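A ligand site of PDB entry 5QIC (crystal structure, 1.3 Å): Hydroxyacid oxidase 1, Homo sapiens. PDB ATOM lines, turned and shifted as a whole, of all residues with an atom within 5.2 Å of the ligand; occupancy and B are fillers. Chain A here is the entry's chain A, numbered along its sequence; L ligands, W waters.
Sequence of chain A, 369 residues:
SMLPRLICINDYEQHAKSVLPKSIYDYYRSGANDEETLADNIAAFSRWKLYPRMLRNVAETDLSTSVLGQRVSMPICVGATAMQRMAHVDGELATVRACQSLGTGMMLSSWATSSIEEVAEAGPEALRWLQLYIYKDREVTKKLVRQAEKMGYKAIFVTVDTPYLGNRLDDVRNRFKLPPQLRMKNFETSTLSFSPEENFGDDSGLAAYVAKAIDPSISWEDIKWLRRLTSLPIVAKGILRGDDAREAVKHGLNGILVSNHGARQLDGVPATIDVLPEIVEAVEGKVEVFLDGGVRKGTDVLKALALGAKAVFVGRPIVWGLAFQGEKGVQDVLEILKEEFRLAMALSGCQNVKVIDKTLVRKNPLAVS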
ATOM      1  N   TYR A  27       8.511  14.812  17.677  1.00  0.00           N
ATOM      2  CA  TYR A  27       8.983  13.733  16.839  1.00  0.00           C
ATOM      3  C   TYR A  27      10.507  13.846  16.625  1.00  0.00           C
ATOM      4  O   TYR A  27      11.255  12.868  16.780  1.00  0.00           O
ATOM      5  CB  TYR A  27       8.231  13.649  15.486  1.00  0.00           C
ATOM      6  CG  TYR A  27       8.919  12.734  14.531  1.00  0.00           C
ATOM      7  CD1 TYR A  27       8.943  11.369  14.719  1.00  0.00           C
ATOM      8  CD2 TYR A  27       9.732  13.238  13.483  1.00  0.00           C
ATOM      9  CE1 TYR A  27       9.667  10.531  13.902  1.00  0.00           C
ATOM     10  CE2 TYR A  27      10.456  12.384  12.651  1.00  0.00           C
ATOM     11  CZ  TYR A  27      10.418  11.055  12.823  1.00  0.00           C
ATOM     12  OH  TYR A  27      11.184  10.188  12.078  1.00  0.00           O
ATOM     13  N   TYR A  28      10.940  15.070  16.284  1.00  0.00           N
ATOM     14  CA  TYR A  28      12.354  15.301  15.965  1.00  0.00           C
ATOM     15  C   TYR A  28      13.238  15.278  17.240  1.00  0.00           C
ATOM     16  O   TYR A  28      14.359  14.702  17.235  1.00  0.00           O
ATOM     17  CB  TYR A  28      12.508  16.611  15.253  1.00  0.00           C
ATOM     18  CG  TYR A  28      11.945  16.739  13.857  1.00  0.00           C
ATOM     19  CD1 TYR A  28      12.218  15.809  12.888  1.00  0.00           C
ATOM     20  CD2 TYR A  28      11.233  17.898  13.487  1.00  0.00           C
ATOM     21  CE1 TYR A  28      11.703  15.964  11.527  1.00  0.00           C
ATOM     22  CE2 TYR A  28      10.772  18.057  12.174  1.00  0.00           C
ATOM     23  CZ  TYR A  28      11.001  17.089  11.261  1.00  0.00           C
ATOM     24  OH  TYR A  28      10.597  17.269   9.934  1.00  0.00           O
ATOM     25  N   ASN A  41      24.329  11.699  25.455  1.00  0.00           N
ATOM     26  CA  ASN A  41      25.058  11.976  24.244  1.00  0.00           C
ATOM     27  C   ASN A  41      25.667  13.368  24.246  1.00  0.00           C
ATOM     28  O   ASN A  41      26.773  13.539  23.698  1.00  0.00           O
ATOM     29  CB  ASN A  41      24.141  11.834  23.008  1.00  0.00           C
ATOM     30  CG  ASN A  41      23.991  10.413  22.493  1.00  0.00           C
ATOM     31  OD1 ASN A  41      24.673   9.484  22.968  1.00  0.00           O
ATOM     32  ND2 ASN A  41      23.044  10.238  21.558  1.00  0.00           N
ATOM     33  N   GLY A  79      23.728  13.372   8.625  1.00  0.00           N
ATOM     34  CA  GLY A  79      23.108  12.078   8.873  1.00  0.00           C
ATOM     35  C   GLY A  79      21.711  11.958   8.419  1.00  0.00           C
ATOM     36  O   GLY A  79      20.996  12.927   8.266  1.00  0.00           O
ATOM     37  N   ALA A  80      21.260  10.691   8.264  1.00  0.00           N
ATOM     38  CA  ALA A  80      19.895  10.376   7.823  1.00  0.00           C
ATOM     39  C   ALA A  80      18.868  10.772   8.866  1.00  0.00           C
ATOM     40  O   ALA A  80      18.934  10.325  10.027  1.00  0.00           O
ATOM     41  CB  ALA A  80      19.759   8.893   7.502  1.00  0.00           C
ATOM     42  N   THR A  81      17.914  11.625   8.532  1.00  0.00           N
ATOM     43  CA  THR A  81      16.803  11.935   9.389  1.00  0.00           C
ATOM     44  C   THR A  81      15.579  11.849   8.525  1.00  0.00           C
ATOM     45  O   THR A  81      15.524  12.496   7.441  1.00  0.00           O
ATOM     46  CB  THR A  81      16.892  13.315  10.074  1.00  0.00           C
ATOM     47  OG1 THR A  81      17.245  14.315   9.121  1.00  0.00           O
ATOM     48  CG2 THR A  81      17.902  13.379  11.146  1.00  0.00           C
ATOM     49  N   ALA A  82      14.627  11.032   8.905  1.00  0.00           N
ATOM     50  CA  ALA A  82      13.391  10.854   8.153  1.00  0.00           C
ATOM     51  C   ALA A  82      12.531  12.072   8.061  1.00  0.00           C
ATOM     52  O   ALA A  82      12.532  12.923   8.917  1.00  0.00           O
ATOM     53  CB  ALA A  82      12.561   9.746   8.786  1.00  0.00           C
ATOM     54  N   SER A 109      18.038   9.181   4.124  1.00  0.00           N
ATOM     55  CA  SER A 109      17.180   8.213   4.775  1.00  0.00           C
ATOM     56  C   SER A 109      16.455   7.303   3.818  1.00  0.00           C
ATOM     57  O   SER A 109      15.932   7.778   2.815  1.00  0.00           O
ATOM     58  CB  SER A 109      16.117   8.925   5.595  1.00  0.00           C
ATOM     59  OG  SER A 109      15.283   7.939   6.233  1.00  0.00           O
ATOM     60  N   SER A 110      14.919   9.494   4.146  1.00  0.00           N
ATOM     61  CA  SER A 110      13.535   9.576   3.641  1.00  0.00           C
ATOM     62  C   SER A 110      12.738   8.320   3.993  1.00  0.00           C
ATOM     63  O   SER A 110      11.726   8.021   3.354  1.00  0.00           O
ATOM     64  CB  SER A 110      13.503   9.874   2.135  1.00  0.00           C
ATOM     65  N   TRP A 111      13.165   7.619   5.053  1.00  0.00           N
ATOM     66  CA  TRP A 111      12.804   6.230   5.306  1.00  0.00           C
ATOM     67  C   TRP A 111      12.939   5.368   4.047  1.00  0.00           C
ATOM     68  O   TRP A 111      13.969   5.399   3.379  1.00  0.00           O
ATOM     69  CB  TRP A 111      11.389   6.125   5.879  1.00  0.00           C
ATOM     70  CG  TRP A 111      11.027   4.751   6.326  1.00  0.00           C
ATOM     71  CD1 TRP A 111      10.579   3.722   5.545  1.00  0.00           C
ATOM     72  CD2 TRP A 111      11.054   4.243   7.670  1.00  0.00           C
ATOM     73  NE1 TRP A 111      10.338   2.604   6.311  1.00  0.00           N
ATOM     74  CE2 TRP A 111      10.625   2.896   7.616  1.00  0.00           C
ATOM     75  CE3 TRP A 111      11.417   4.798   8.906  1.00  0.00           C
ATOM     76  CZ2 TRP A 111      10.542   2.097   8.746  1.00  0.00           C
ATOM     77  CZ3 TRP A 111      11.329   3.993  10.042  1.00  0.00           C
ATOM     78  CH2 TRP A 111      10.900   2.660   9.954  1.00  0.00           C
ATOM     79  N   GLN A 131      21.221   5.621   3.297  1.00  0.00           N
ATOM     80  CA  GLN A 131      20.946   4.779   4.486  1.00  0.00           C
ATOM     81  C   GLN A 131      19.849   3.783   4.131  1.00  0.00           C
ATOM     82  O   GLN A 131      18.801   4.162   3.610  1.00  0.00           O
ATOM     83  CB  GLN A 131      20.544   5.648   5.631  1.00  0.00           C
ATOM     84  CG  GLN A 131      20.110   4.913   6.909  1.00  0.00           C
ATOM     85  CD  GLN A 131      18.662   4.482   6.921  1.00  0.00           C
ATOM     86  OE1 GLN A 131      17.810   5.318   6.687  1.00  0.00           O
ATOM     87  NE2 GLN A 131      18.382   3.207   7.256  1.00  0.00           N
ATOM     88  N   TYR A 133      17.503   0.351   5.328  1.00  0.00           N
ATOM     89  CA  TYR A 133      17.016  -0.717   6.186  1.00  0.00           C
ATOM     90  C   TYR A 133      16.815  -1.997   5.344  1.00  0.00           C
ATOM     91  O   TYR A 133      16.433  -1.885   4.147  1.00  0.00           O
ATOM     92  CB  TYR A 133      15.678  -0.321   6.761  1.00  0.00           C
ATOM     93  CG  TYR A 133      15.723   0.726   7.896  1.00  0.00           C
ATOM     94  CD1 TYR A 133      16.335   0.436   9.073  1.00  0.00           C
ATOM     95  CD2 TYR A 133      15.192   1.979   7.734  1.00  0.00           C
ATOM     96  CE1 TYR A 133      16.412   1.396  10.067  1.00  0.00           C
ATOM     97  CE2 TYR A 133      15.283   2.956   8.724  1.00  0.00           C
ATOM     98  CZ  TYR A 133      15.859   2.592   9.913  1.00  0.00           C
ATOM     99  OH  TYR A 133      15.931   3.515  10.931  1.00  0.00           O
ATOM    100  N   THR A 159      21.536   0.375   8.490  1.00  0.00           N
ATOM    101  CA  THR A 159      21.217   0.530   9.911  1.00  0.00           C
ATOM    102  C   THR A 159      20.919  -0.796  10.539  1.00  0.00           C
ATOM    103  O   THR A 159      20.064  -1.563   9.991  1.00  0.00           O
ATOM    104  CB  THR A 159      20.033   1.500  10.040  1.00  0.00           C
ATOM    105  OG1 THR A 159      20.432   2.746   9.448  1.00  0.00           O
ATOM    106  CG2 THR A 159      19.639   1.676  11.485  1.00  0.00           C
ATOM    107  N   LYS A 237      25.822   0.901  10.516  1.00  0.00           N
ATOM    108  CA  LYS A 237      25.375   2.043  11.356  1.00  0.00           C
ATOM    109  C   LYS A 237      24.594   1.562  12.551  1.00  0.00           C
ATOM    110  O   LYS A 237      23.560   0.878  12.409  1.00  0.00           O
ATOM    111  CB  LYS A 237      24.542   2.976  10.484  1.00  0.00           C
ATOM    112  CG  LYS A 237      23.840   4.123  11.218  1.00  0.00           C
ATOM    113  CD  LYS A 237      23.049   5.013  10.288  1.00  0.00           C
ATOM    114  CE  LYS A 237      22.476   6.267  10.907  1.00  0.00           C
ATOM    115  NZ  LYS A 237      21.311   5.979  11.732  1.00  0.00           N
ATOM    116  N   SER A 259      26.900   4.710  16.690  1.00  0.00           N
ATOM    117  CA  SER A 259      25.636   5.395  16.764  1.00  0.00           C
ATOM    118  C   SER A 259      24.731   4.654  17.682  1.00  0.00           C
ATOM    119  O   SER A 259      24.728   3.412  17.708  1.00  0.00           O
ATOM    120  CB  SER A 259      25.014   5.436  15.349  1.00  0.00           C
ATOM    121  OG  SER A 259      23.749   6.056  15.360  1.00  0.00           O
ATOM    122  N   HIS A 261      21.552   5.753  17.389  1.00  0.00           N
ATOM    123  CA  HIS A 261      20.329   6.154  16.663  1.00  0.00           C
ATOM    124  C   HIS A 261      19.748   7.447  17.249  1.00  0.00           C
ATOM    125  O   HIS A 261      18.539   7.619  17.401  1.00  0.00           O
ATOM    126  CB  HIS A 261      19.304   5.028  16.630  1.00  0.00           C
ATOM    127  CG  HIS A 261      18.359   5.026  15.476  1.00  0.00           C
ATOM    128  ND1 HIS A 261      18.329   3.951  14.604  1.00  0.00           N
ATOM    129  CD2 HIS A 261      17.375   5.874  15.097  1.00  0.00           C
ATOM    130  CE1 HIS A 261      17.359   4.187  13.712  1.00  0.00           C
ATOM    131  NE2 HIS A 261      16.739   5.321  13.996  1.00  0.00           N
ATOM    132  N   GLY A 262      20.632   8.373  17.636  1.00  0.00           N
ATOM    133  CA  GLY A 262      20.195   9.620  18.230  1.00  0.00           C
ATOM    134  C   GLY A 262      19.473   9.367  19.551  1.00  0.00           C
ATOM    135  O   GLY A 262      18.612  10.164  19.954  1.00  0.00           O
ATOM    136  N   ARG A 264      17.318   7.086  20.265  1.00  0.00           N
ATOM    137  CA  ARG A 264      15.933   6.793  19.960  1.00  0.00           C
ATOM    138  C   ARG A 264      15.595   5.322  19.973  1.00  0.00           C
ATOM    139  O   ARG A 264      14.390   5.011  19.716  1.00  0.00           O
ATOM    140  CB  ARG A 264      15.536   7.389  18.594  1.00  0.00           C
ATOM    141  CG  ARG A 264      15.676   8.920  18.592  1.00  0.00           C
ATOM    142  CD  ARG A 264      15.709   9.547  17.235  1.00  0.00           C
ATOM    143  NE  ARG A 264      14.488   9.512  16.440  1.00  0.00           N
ATOM    144  CZ  ARG A 264      13.499  10.403  16.520  1.00  0.00           C
ATOM    145  NH1 ARG A 264      13.535  11.391  17.378  1.00  0.00           N
ATOM    146  NH2 ARG A 264      12.452  10.374  15.648  1.00  0.00           N
ATOM    147  N   ASP A 292      28.015   9.492  15.341  1.00  0.00           N
ATOM    148  CA  ASP A 292      26.927  10.452  15.441  1.00  0.00           C
ATOM    149  C   ASP A 292      26.333  10.339  16.842  1.00  0.00           C
ATOM    150  O   ASP A 292      26.682   9.417  17.604  1.00  0.00           O
ATOM    151  CB  ASP A 292      25.856  10.298  14.327  1.00  0.00           C
ATOM    152  CG  ASP A 292      25.055   9.082  14.389  1.00  0.00           C
ATOM    153  OD1 ASP A 292      24.820   8.491  15.419  1.00  0.00           O
ATOM    154  OD2 ASP A 292      24.503   8.694  13.324  1.00  0.00           O
ATOM    155  N   GLY A 293      25.504  11.331  17.187  1.00  0.00           N
ATOM    156  CA  GLY A 293      24.893  11.385  18.496  1.00  0.00           C
ATOM    157  C   GLY A 293      25.442  12.522  19.353  1.00  0.00           C
ATOM    158  O   GLY A 293      26.479  12.349  19.971  1.00  0.00           O
ATOM    159  N   GLY A 294      24.691  13.621  19.444  1.00  0.00           N
ATOM    160  CA  GLY A 294      25.078  14.672  20.344  1.00  0.00           C
ATOM    161  C   GLY A 294      26.049  15.683  19.813  1.00  0.00           C
ATOM    162  O   GLY A 294      26.416  16.569  20.581  1.00  0.00           O
ATOM    163  N   VAL A 295      26.404  15.681  18.523  1.00  0.00           N
ATOM    164  CA  VAL A 295      27.337  16.662  17.979  1.00  0.00           C
ATOM    165  C   VAL A 295      26.566  17.972  17.775  1.00  0.00           C
ATOM    166  O   VAL A 295      25.619  18.016  16.974  1.00  0.00           O
ATOM    167  CB  VAL A 295      27.978  16.174  16.675  1.00  0.00           C
ATOM    168  CG1 VAL A 295      28.784  17.268  16.024  1.00  0.00           C
ATOM    169  CG2 VAL A 295      28.778  14.915  16.872  1.00  0.00           C
ATOM    170  N   ARG A 296      27.003  19.019  18.500  1.00  0.00           N
ATOM    171  CA  ARG A 296      26.375  20.361  18.460  1.00  0.00           C
ATOM    172  C   ARG A 296      27.356  21.464  18.287  1.00  0.00           C
ATOM    173  O   ARG A 296      26.935  22.568  17.907  1.00  0.00           O
ATOM    174  CB  ARG A 296      25.598  20.590  19.707  1.00  0.00           C
ATOM    175  CG  ARG A 296      24.581  19.522  20.080  1.00  0.00           C
ATOM    176  CD  ARG A 296      23.388  19.458  19.149  1.00  0.00           C
ATOM    177  NE  ARG A 296      22.432  18.386  19.519  1.00  0.00           N
ATOM    178  CZ  ARG A 296      22.353  17.222  18.940  1.00  0.00           C
ATOM    179  NH1 ARG A 296      23.126  16.879  17.903  1.00  0.00           N
ATOM    180  NH2 ARG A 296      21.394  16.365  19.309  1.00  0.00           N
ATOM    181  N   PHE A 313      28.682  12.721  11.928  1.00  0.00           N
ATOM    182  CA  PHE A 313      27.396  12.999  11.307  1.00  0.00           C
ATOM    183  C   PHE A 313      26.514  13.743  12.259  1.00  0.00           C
ATOM    184  O   PHE A 313      26.524  13.464  13.473  1.00  0.00           O
ATOM    185  CB  PHE A 313      26.685  11.749  10.775  1.00  0.00           C
ATOM    186  CG  PHE A 313      27.453  11.039   9.682  1.00  0.00           C
ATOM    187  CD1 PHE A 313      27.077  11.205   8.348  1.00  0.00           C
ATOM    188  CD2 PHE A 313      28.551  10.281   9.950  1.00  0.00           C
ATOM    189  CE1 PHE A 313      27.792  10.620   7.333  1.00  0.00           C
ATOM    190  CE2 PHE A 313      29.283   9.701   8.923  1.00  0.00           C
ATOM    191  CZ  PHE A 313      28.875   9.844   7.606  1.00  0.00           C
ATOM    192  N   VAL A 314      25.763  14.699  11.738  1.00  0.00           N
ATOM    193  CA  VAL A 314      24.768  15.446  12.503  1.00  0.00           C
ATOM    194  C   VAL A 314      23.382  15.104  12.050  1.00  0.00           C
ATOM    195  O   VAL A 314      23.105  15.123  10.832  1.00  0.00           O
ATOM    196  CB  VAL A 314      24.998  16.944  12.476  1.00  0.00           C
ATOM    197  CG1 VAL A 314      26.207  17.279  13.426  1.00  0.00           C
ATOM    198  CG2 VAL A 314      25.148  17.525  11.153  1.00  0.00           C
ATOM    199  N   GLY A 315      22.482  14.901  12.998  1.00  0.00           N
ATOM    200  CA  GLY A 315      21.105  14.571  12.711  1.00  0.00           C
ATOM    201  C   GLY A 315      20.203  15.756  12.976  1.00  0.00           C
ATOM    202  O   GLY A 315      19.900  16.545  12.056  1.00  0.00           O
ATOM    203  N   ARG A 316      19.787  15.967  14.208  1.00  0.00           N
ATOM    204  CA  ARG A 316      18.777  16.990  14.549  1.00  0.00           C
ATOM    205  C   ARG A 316      19.203  18.394  14.102  1.00  0.00           C
ATOM    206  O   ARG A 316      18.308  19.114  13.654  1.00  0.00           O
ATOM    207  CB  ARG A 316      18.506  16.938  16.032  1.00  0.00           C
ATOM    208  CG  ARG A 316      17.726  15.702  16.451  1.00  0.00           C
ATOM    209  CD  ARG A 316      17.528  15.644  17.940  1.00  0.00           C
ATOM    210  NE  ARG A 316      16.896  14.414  18.372  1.00  0.00           N
ATOM    211  CZ  ARG A 316      17.541  13.330  18.794  1.00  0.00           C
ATOM    212  NH1 ARG A 316      18.844  13.241  18.736  1.00  0.00           N
ATOM    213  NH2 ARG A 316      16.843  12.305  19.325  1.00  0.00           N
ATOM    214  N   PRO A 317      20.478  18.804  14.238  1.00  0.00           N
ATOM    215  CA  PRO A 317      20.814  20.225  13.864  1.00  0.00           C
ATOM    216  C   PRO A 317      20.358  20.530  12.423  1.00  0.00           C
ATOM    217  O   PRO A 317      19.972  21.691  12.144  1.00  0.00           O
ATOM    218  CB  PRO A 317      22.282  20.258  14.031  1.00  0.00           C
ATOM    219  CG  PRO A 317      22.499  19.382  15.249  1.00  0.00           C
ATOM    220  CD  PRO A 317      21.652  18.187  14.904  1.00  0.00           C
HETATM  221  N1  LIG L   1      18.555   6.853  11.352  1.00  0.00           N
HETATM  222  C1  LIG L   1      18.333   6.094  10.258  1.00  0.00           C
HETATM  223  O1  LIG L   1      19.131   5.159  10.058  1.00  0.00           O
HETATM  224  N2  LIG L   1      17.302   6.334   9.419  1.00  0.00           N
HETATM  225  C2  LIG L   1      16.376   7.239   9.599  1.00  0.00           C
HETATM  226  O2  LIG L   1      15.448   7.416   8.798  1.00  0.00           O
HETATM  227  C3  LIG L   1      16.470   8.111  10.764  1.00  0.00           C
HETATM  228  N3  LIG L   1      15.556   9.078  11.015  1.00  0.00           N
HETATM  229  C4  LIG L   1      15.734   9.878  12.080  1.00  0.00           C
HETATM  230  C5  LIG L   1      14.797  10.895  12.312  1.00  0.00           C
HETATM  231  C6  LIG L   1      14.980  11.717  13.388  1.00  0.00           C
HETATM  232  C7  LIG L   1      14.033  12.817  13.676  1.00  0.00           C
HETATM  233  C8  LIG L   1      16.152  11.630  14.217  1.00  0.00           C
HETATM  234  C9  LIG L   1      16.365  12.599  15.379  1.00  0.00           C
HETATM  235  C10 LIG L   1      17.065  10.631  13.999  1.00  0.00           C
HETATM  236  C11 LIG L   1      16.914   9.723  12.947  1.00  0.00           C
HETATM  237  N4  LIG L   1      17.818   8.665  12.680  1.00  0.00           N
HETATM  238  C12 LIG L   1      17.624   7.815  11.601  1.00  0.00           C
HETATM  239  C13 LIG L   1      19.081   8.563  13.422  1.00  0.00           C
HETATM  240  C14 LIG L   1      20.104   9.543  12.821  1.00  0.00           C
HETATM  241  O3  LIG L   1      20.598   9.004  11.557  1.00  0.00           O
HETATM  242  C15 LIG L   1      21.323   9.812  13.666  1.00  0.00           C
HETATM  243  O4  LIG L   1      21.850   8.538  14.146  1.00  0.00           O
HETATM  244  C16 LIG L   1      21.047  10.706  14.875  1.00  0.00           C
HETATM  245  O5  LIG L   1      20.114  11.773  14.491  1.00  0.00           O
HETATM  246  C17 LIG L   1      22.297  11.339  15.371  1.00  0.00           C
HETATM  247  O6  LIG L   1      22.151  12.078  16.583  1.00  0.00           O
HETATM  248  P1  LIG L   1      21.886  13.685  16.647  1.00  0.00           P
HETATM  249  O7  LIG L   1      22.833  14.399  15.737  1.00  0.00           O
HETATM  250  O8  LIG L   1      22.138  13.935  18.109  1.00  0.00           O
HETATM  251  O9  LIG L   1      20.469  13.918  16.232  1.00  0.00           O
HETATM  252  O   HOH W   1      25.443  13.914  16.056  1.00  0.00           O
HETATM  253  O   HOH W   2      23.429   9.562  10.823  1.00  0.00           O
HETATM  254  O   HOH W   3      21.396  12.237  20.220  1.00  0.00           O
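The backbone carbonyl oxygen of Ala 80 is in hydrogen-bond range of an oxygen (O3) of the ligand (2.6 Å). The side-chain hydroxyl (OG) of Ser 109 is in hydrogen-bond range of an oxygen (O2) of the ligand (2.6 Å). An oxygen (O4) of the ligand lies within hydrogen-bond range of the side-chain carboxylate (OD2) of Asp 292, at 2.8 Å. The backbone NH of Gly 315 lies within hydrogen-bond range of an oxygen (O7) of the ligand (2.8 Å). An oxygen (O1) of the ligand lies within hydrogen-bond range of the side-chain hydroxyl of Thr 159, at 2.8 Å. The guanidinium group (NH2) of Arg 296 lies within salt-bridge range of an oxygen (O8) of the ligand, at 2.8 Å. NZ of Lys 237 lies within hydrogen-bond range of O1 of the ligand (2.9 Å). The backbone NH of Gly 294 lies within hydrogen-bond range of an oxygen (O8) of the ligand (2.9 Å). The side-chain amide oxygen (OE1) of Gln 131 is in hydrogen-bond range of a nitrogen (N2) of the ligand. The backbone NH (N) of Arg 316 lies within hydrogen-bond range of an oxygen (O9) of the ligand (3.0 Å). NH1 of Arg 316 lies within salt-bridge range of O9 of the ligand, at 3.1 Å. The backbone NH (N) of Ala 82 sits at hydrogen-bond distance from a nitrogen (N3) of the ligand (3.0 Å). An oxygen (O4) of the ligand sits at hydrogen-bond distance from the side-chain hydroxyl (OG) of Ser 259 (3.4 Å). N of Gly 293 lies close to O6 of the ligand, 3.5 Å away. The side-chain hydroxyl of Tyr 133 sits at hydrogen-bond distance from a nitrogen (N2) of the ligand (3.5 Å).
OG of Ser 109 sits at hydrogen-bond distance from N of Trp 111 (2.4 Å). The side-chain carboxylate (OD1) of Asp 292 lies within hydrogen-bond range of the side-chain hydroxyl (OG) of Ser 259. The side-chain amide nitrogen (NE2) of Gln 131 lies within hydrogen-bond range of the side-chain hydroxyl (OG1) of Thr 159 (3.0 Å). The backbone carbonyl oxygen (O) of Tyr 28 lies within hydrogen-bond range of the guanidinium group (NE) of Arg 316. The backbone carbonyl oxygen (O) of Gly 262 is in hydrogen-bond range of the guanidinium group (NH2) of Arg 316 (2.8 Å). The backbone carbonyl oxygen of Tyr 28 lies within hydrogen-bond range of the guanidinium group of Arg 264 (3.4 Å). NH1 of Arg 264 is in hydrogen-bond range of O of Tyr 27 (2.8 Å). The backbone carbonyl oxygen (O) of Val 314 sits at hydrogen-bond distance from the backbone NH (N) of Gly 79, at 2.9 Å.
Merely in contact with the ligand: Tyr 28 (3.4 Å), Arg 264 (3.5 Å), Thr 81 (3.5 Å), Gly 262 (3.5 Å), His 261 (3.6 Å), Tyr 27 (3.7 Å) and Val 314 (3.8 Å). Hydrophobic or aromatic side chains that line the ligand: Tyr 27, Tyr 28, Ala 82, Tyr 133 and His 261. Of the 28 residues printed, 21 come within 4 Å of the ligand.
Water W3 lies within hydrogen-bond range of O8 of the ligand (2.8 Å), ND2 of Asn 41 (2.9 Å), NH1 of Arg 316 (3.1 Å) and O of Gly 262 (3.5 Å). Water W2 lies within hydrogen-bond range of the side-chain carboxylate (OD2) of Asp 292 (2.9 Å) and an oxygen (O3) of the ligand (3.0 Å).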
